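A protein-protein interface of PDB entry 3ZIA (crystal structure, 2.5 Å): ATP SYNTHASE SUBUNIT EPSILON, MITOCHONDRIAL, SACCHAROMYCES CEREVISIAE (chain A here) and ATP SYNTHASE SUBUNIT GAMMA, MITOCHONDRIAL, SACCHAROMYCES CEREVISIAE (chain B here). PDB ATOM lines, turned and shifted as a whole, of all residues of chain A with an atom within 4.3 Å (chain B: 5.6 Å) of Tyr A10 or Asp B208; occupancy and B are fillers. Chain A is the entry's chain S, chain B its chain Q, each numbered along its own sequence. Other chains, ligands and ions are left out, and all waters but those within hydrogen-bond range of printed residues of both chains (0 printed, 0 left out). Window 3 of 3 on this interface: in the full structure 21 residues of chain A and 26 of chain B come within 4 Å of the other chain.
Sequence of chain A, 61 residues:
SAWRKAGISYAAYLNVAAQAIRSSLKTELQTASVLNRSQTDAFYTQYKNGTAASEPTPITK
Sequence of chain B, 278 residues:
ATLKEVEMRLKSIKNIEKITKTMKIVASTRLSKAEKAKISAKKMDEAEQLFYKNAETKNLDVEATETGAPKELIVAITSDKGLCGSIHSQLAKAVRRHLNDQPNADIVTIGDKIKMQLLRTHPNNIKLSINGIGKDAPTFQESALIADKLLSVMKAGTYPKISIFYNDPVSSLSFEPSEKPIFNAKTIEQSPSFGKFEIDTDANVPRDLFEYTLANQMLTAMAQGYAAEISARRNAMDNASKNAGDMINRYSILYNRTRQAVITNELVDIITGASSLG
N of Tyr A10 sits at hydrogen-bond distance from OE1 of Glu B211 (3.1 Å).
Glu B211 touches Ser A9 (OE1 to CB, 3.9 Å).
Asp B208 touches Tyr A10 (OD2 to CD1, 3.3 Å).
Tyr A10 touches Tyr B212.
CD1 of Tyr B212 touches CD1 of Leu A14 (3.8 Å).
Of the 10 printed residues of chain B, 3 touch a printed residue of chain A.
Hydrophobic or aromatic side chains of chain A that line the printed part of chain B: Tyr A10 and Leu A14.
Among the printed residues, no Asp or Glu carboxylate lies within 4 Å of a Lys or Arg side-chain nitrogen of the other chain.
NE of Arg B207 lies within salt-bridge range of OE2 of Glu B211 (3.5 Å).
Of the printed residues of chain B, Ser A9 touches Glu B211 (3.9 Å).
Printed residues of chain B within 4 Å of Tyr A10: Asp B208 (3.3 Å), Glu B211 (3.1 Å) and Tyr B212 (3.99 Å).
Printed residues of chain B within 4 Å of Leu A14: Tyr B212 (3.8 Å).
Printed residues of chain A within 4 Å of Glu B211: Ser A9 (3.9 Å) and Tyr A10 (3.1 Å).
Printed residues of chain A within 4 Å of Tyr B212: Tyr A10 and Leu A14.
The nearest printed residue of chain A that does not touch Asp B208 is Ala A11 (6.3 Å).
The nearest printed residue of chain A that does not touch Glu B211 is Ala A11 (4.03 Å).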
ATOM      1  N   SER A   9       1.311 -25.030  16.010  1.00  0.00           N
ATOM      2  CA  SER A   9       0.688 -24.342  14.893  1.00  0.00           C
ATOM      3  C   SER A   9       1.172 -24.961  13.589  1.00  0.00           C
ATOM      4  O   SER A   9       2.145 -25.709  13.580  1.00  0.00           O
ATOM      5  CB  SER A   9       1.046 -22.859  14.935  1.00  0.00           C
ATOM      6  OG  SER A   9       2.447 -22.674  14.804  1.00  0.00           O
ATOM      7  N   TYR A  10       0.502 -24.635  12.488  1.00  0.00           N
ATOM      8  CA  TYR A  10       0.793 -25.264  11.201  1.00  0.00           C
ATOM      9  C   TYR A  10       2.245 -25.090  10.754  1.00  0.00           C
ATOM     10  O   TYR A  10       2.910 -26.066  10.397  1.00  0.00           O
ATOM     11  CB  TYR A  10      -0.174 -24.777  10.114  1.00  0.00           C
ATOM     12  CG  TYR A  10       0.006 -25.467   8.773  1.00  0.00           C
ATOM     13  CD1 TYR A  10      -0.370 -26.801   8.589  1.00  0.00           C
ATOM     14  CD2 TYR A  10       0.548 -24.786   7.687  1.00  0.00           C
ATOM     15  CE1 TYR A  10      -0.204 -27.434   7.354  1.00  0.00           C
ATOM     16  CE2 TYR A  10       0.712 -25.408   6.452  1.00  0.00           C
ATOM     17  CZ  TYR A  10       0.340 -26.730   6.291  1.00  0.00           C
ATOM     18  OH  TYR A  10       0.509 -27.339   5.066  1.00  0.00           O
ATOM     19  N   ALA A  11       2.733 -23.852  10.779  1.00  0.00           N
ATOM     20  CA  ALA A  11       4.089 -23.554  10.311  1.00  0.00           C
ATOM     21  C   ALA A  11       5.168 -24.125  11.238  1.00  0.00           C
ATOM     22  O   ALA A  11       6.220 -24.558  10.762  1.00  0.00           O
ATOM     23  CB  ALA A  11       4.273 -22.061  10.118  1.00  0.00           C
ATOM     24  N   ALA A  12       4.896 -24.128  12.546  1.00  0.00           N
ATOM     25  CA  ALA A  12       5.780 -24.752  13.540  1.00  0.00           C
ATOM     26  C   ALA A  12       5.967 -26.245  13.269  1.00  0.00           C
ATOM     27  O   ALA A  12       7.070 -26.782  13.430  1.00  0.00           O
ATOM     28  CB  ALA A  12       5.242 -24.539  14.951  1.00  0.00           C
ATOM     29  N   TYR A  13       4.875 -26.893  12.861  1.00  0.00           N
ATOM     30  CA  TYR A  13       4.882 -28.280  12.413  1.00  0.00           C
ATOM     31  C   TYR A  13       5.803 -28.482  11.203  1.00  0.00           C
ATOM     32  O   TYR A  13       6.660 -29.381  11.210  1.00  0.00           O
ATOM     33  CB  TYR A  13       3.442 -28.747  12.121  1.00  0.00           C
ATOM     34  CG  TYR A  13       3.303 -29.785  11.023  1.00  0.00           C
ATOM     35  CD1 TYR A  13       3.687 -31.119  11.234  1.00  0.00           C
ATOM     36  CD2 TYR A  13       2.776 -29.440   9.777  1.00  0.00           C
ATOM     37  CE1 TYR A  13       3.568 -32.077  10.221  1.00  0.00           C
ATOM     38  CE2 TYR A  13       2.646 -30.389   8.759  1.00  0.00           C
ATOM     39  CZ  TYR A  13       3.043 -31.703   8.989  1.00  0.00           C
ATOM     40  OH  TYR A  13       2.914 -32.640   7.989  1.00  0.00           O
ATOM     41  N   LEU A  14       5.630 -27.645  10.181  1.00  0.00           N
ATOM     42  CA  LEU A  14       6.424 -27.738   8.956  1.00  0.00           C
ATOM     43  C   LEU A  14       7.912 -27.545   9.219  1.00  0.00           C
ATOM     44  O   LEU A  14       8.757 -28.170   8.576  1.00  0.00           O
ATOM     45  CB  LEU A  14       5.956 -26.703   7.942  1.00  0.00           C
ATOM     46  CG  LEU A  14       4.537 -26.828   7.405  1.00  0.00           C
ATOM     47  CD1 LEU A  14       4.167 -25.551   6.688  1.00  0.00           C
ATOM     48  CD2 LEU A  14       4.411 -28.034   6.483  1.00  0.00           C
ATOM     49  N   ASN B 204      -9.352 -28.407   7.540  1.00  0.00           N
ATOM     50  CA  ASN B 204      -8.983 -27.015   7.793  1.00  0.00           C
ATOM     51  C   ASN B 204      -8.034 -26.434   6.748  1.00  0.00           C
ATOM     52  O   ASN B 204      -6.823 -26.654   6.809  1.00  0.00           O
ATOM     53  CB  ASN B 204      -8.386 -26.868   9.191  1.00  0.00           C
ATOM     54  CG  ASN B 204      -9.420 -26.495  10.221  1.00  0.00           C
ATOM     55  OD1 ASN B 204      -9.778 -25.328  10.356  1.00  0.00           O
ATOM     56  ND2 ASN B 204      -9.904 -27.485  10.960  1.00  0.00           N
ATOM     57  N   VAL B 205      -8.595 -25.702   5.789  1.00  0.00           N
ATOM     58  CA  VAL B 205      -7.804 -25.009   4.772  1.00  0.00           C
ATOM     59  C   VAL B 205      -7.661 -23.511   5.086  1.00  0.00           C
ATOM     60  O   VAL B 205      -6.608 -22.931   4.804  1.00  0.00           O
ATOM     61  CB  VAL B 205      -8.364 -25.222   3.335  1.00  0.00           C
ATOM     62  CG1 VAL B 205      -7.485 -24.532   2.285  1.00  0.00           C
ATOM     63  CG2 VAL B 205      -8.481 -26.706   3.018  1.00  0.00           C
ATOM     64  N   PRO B 206      -8.708 -22.881   5.674  1.00  0.00           N
ATOM     65  CA  PRO B 206      -8.612 -21.447   5.955  1.00  0.00           C
ATOM     66  C   PRO B 206      -7.588 -21.150   7.047  1.00  0.00           C
ATOM     67  O   PRO B 206      -6.697 -20.321   6.842  1.00  0.00           O
ATOM     68  CB  PRO B 206     -10.027 -21.075   6.433  1.00  0.00           C
ATOM     69  CG  PRO B 206     -10.897 -22.230   6.061  1.00  0.00           C
ATOM     70  CD  PRO B 206     -10.004 -23.422   6.124  1.00  0.00           C
ATOM     71  N   ARG B 207      -7.715 -21.834   8.183  1.00  0.00           N
ATOM     72  CA  ARG B 207      -6.813 -21.655   9.318  1.00  0.00           C
ATOM     73  C   ARG B 207      -5.358 -21.915   8.933  1.00  0.00           C
ATOM     74  O   ARG B 207      -4.473 -21.114   9.245  1.00  0.00           O
ATOM     75  CB  ARG B 207      -7.238 -22.550  10.483  1.00  0.00           C
ATOM     76  CG  ARG B 207      -6.368 -22.416  11.718  1.00  0.00           C
ATOM     77  CD  ARG B 207      -7.079 -22.894  12.971  1.00  0.00           C
ATOM     78  NE  ARG B 207      -6.134 -23.025  14.077  1.00  0.00           N
ATOM     79  CZ  ARG B 207      -5.610 -24.177  14.491  1.00  0.00           C
ATOM     80  NH1 ARG B 207      -5.951 -25.318  13.908  1.00  0.00           N
ATOM     81  NH2 ARG B 207      -4.750 -24.188  15.501  1.00  0.00           N
ATOM     82  N   ASP B 208      -5.126 -23.023   8.237  1.00  0.00           N
ATOM     83  CA  ASP B 208      -3.784 -23.409   7.804  1.00  0.00           C
ATOM     84  C   ASP B 208      -3.163 -22.432   6.809  1.00  0.00           C
ATOM     85  O   ASP B 208      -1.959 -22.208   6.837  1.00  0.00           O
ATOM     86  CB  ASP B 208      -3.793 -24.825   7.219  1.00  0.00           C
ATOM     87  CG  ASP B 208      -3.972 -25.901   8.284  1.00  0.00           C
ATOM     88  OD1 ASP B 208      -4.438 -25.585   9.401  1.00  0.00           O
ATOM     89  OD2 ASP B 208      -3.642 -27.071   7.998  1.00  0.00           O
ATOM     90  N   LEU B 209      -3.981 -21.851   5.938  1.00  0.00           N
ATOM     91  CA  LEU B 209      -3.482 -20.874   4.975  1.00  0.00           C
ATOM     92  C   LEU B 209      -3.152 -19.538   5.639  1.00  0.00           C
ATOM     93  O   LEU B 209      -2.206 -18.864   5.241  1.00  0.00           O
ATOM     94  CB  LEU B 209      -4.475 -20.678   3.828  1.00  0.00           C
ATOM     95  CG  LEU B 209      -4.036 -19.819   2.637  1.00  0.00           C
ATOM     96  CD1 LEU B 209      -2.763 -20.350   1.973  1.00  0.00           C
ATOM     97  CD2 LEU B 209      -5.162 -19.727   1.630  1.00  0.00           C
ATOM     98  N   PHE B 210      -3.934 -19.164   6.647  1.00  0.00           N
ATOM     99  CA  PHE B 210      -3.677 -17.950   7.412  1.00  0.00           C
ATOM    100  C   PHE B 210      -2.393 -18.085   8.228  1.00  0.00           C
ATOM    101  O   PHE B 210      -1.574 -17.165   8.263  1.00  0.00           O
ATOM    102  CB  PHE B 210      -4.891 -17.618   8.291  1.00  0.00           C
ATOM    103  CG  PHE B 210      -4.562 -16.879   9.563  1.00  0.00           C
ATOM    104  CD1 PHE B 210      -4.069 -15.576   9.534  1.00  0.00           C
ATOM    105  CD2 PHE B 210      -4.790 -17.481  10.798  1.00  0.00           C
ATOM    106  CE1 PHE B 210      -3.785 -14.894  10.721  1.00  0.00           C
ATOM    107  CE2 PHE B 210      -4.513 -16.812  11.987  1.00  0.00           C
ATOM    108  CZ  PHE B 210      -4.010 -15.514  11.952  1.00  0.00           C
ATOM    109  N   GLU B 211      -2.212 -19.243   8.856  1.00  0.00           N
ATOM    110  CA  GLU B 211      -1.048 -19.493   9.706  1.00  0.00           C
ATOM    111  C   GLU B 211       0.229 -19.681   8.885  1.00  0.00           C
ATOM    112  O   GLU B 211       1.330 -19.413   9.369  1.00  0.00           O
ATOM    113  CB  GLU B 211      -1.289 -20.702  10.614  1.00  0.00           C
ATOM    114  CG  GLU B 211      -2.415 -20.505  11.628  1.00  0.00           C
ATOM    115  CD  GLU B 211      -2.499 -21.615  12.673  1.00  0.00           C
ATOM    116  OE1 GLU B 211      -1.974 -22.722  12.427  1.00  0.00           O
ATOM    117  OE2 GLU B 211      -3.095 -21.381  13.749  1.00  0.00           O
ATOM    118  N   TYR B 212       0.067 -20.132   7.643  1.00  0.00           N
ATOM    119  CA  TYR B 212       1.181 -20.354   6.725  1.00  0.00           C
ATOM    120  C   TYR B 212       1.636 -19.050   6.092  1.00  0.00           C
ATOM    121  O   TYR B 212       2.835 -18.828   5.913  1.00  0.00           O
ATOM    122  CB  TYR B 212       0.762 -21.341   5.639  1.00  0.00           C
ATOM    123  CG  TYR B 212       1.817 -21.700   4.611  1.00  0.00           C
ATOM    124  CD1 TYR B 212       2.936 -22.447   4.962  1.00  0.00           C
ATOM    125  CD2 TYR B 212       1.665 -21.331   3.275  1.00  0.00           C
ATOM    126  CE1 TYR B 212       3.894 -22.795   4.016  1.00  0.00           C
ATOM    127  CE2 TYR B 212       2.614 -21.677   2.319  1.00  0.00           C
ATOM    128  CZ  TYR B 212       3.729 -22.410   2.698  1.00  0.00           C
ATOM    129  OH  TYR B 212       4.678 -22.762   1.762  1.00  0.00           O
ATOM    130  N   THR B 213       0.674 -18.199   5.740  1.00  0.00           N
ATOM    131  CA  THR B 213       0.973 -16.904   5.139  1.00  0.00           C
ATOM    132  C   THR B 213       1.576 -15.971   6.187  1.00  0.00           C
ATOM    133  O   THR B 213       2.532 -15.252   5.888  1.00  0.00           O
ATOM    134  CB  THR B 213      -0.271 -16.274   4.466  1.00  0.00           C
ATOM    135  OG1 THR B 213      -0.852 -17.223   3.562  1.00  0.00           O
ATOM    136  CG2 THR B 213       0.106 -15.026   3.679  1.00  0.00           C
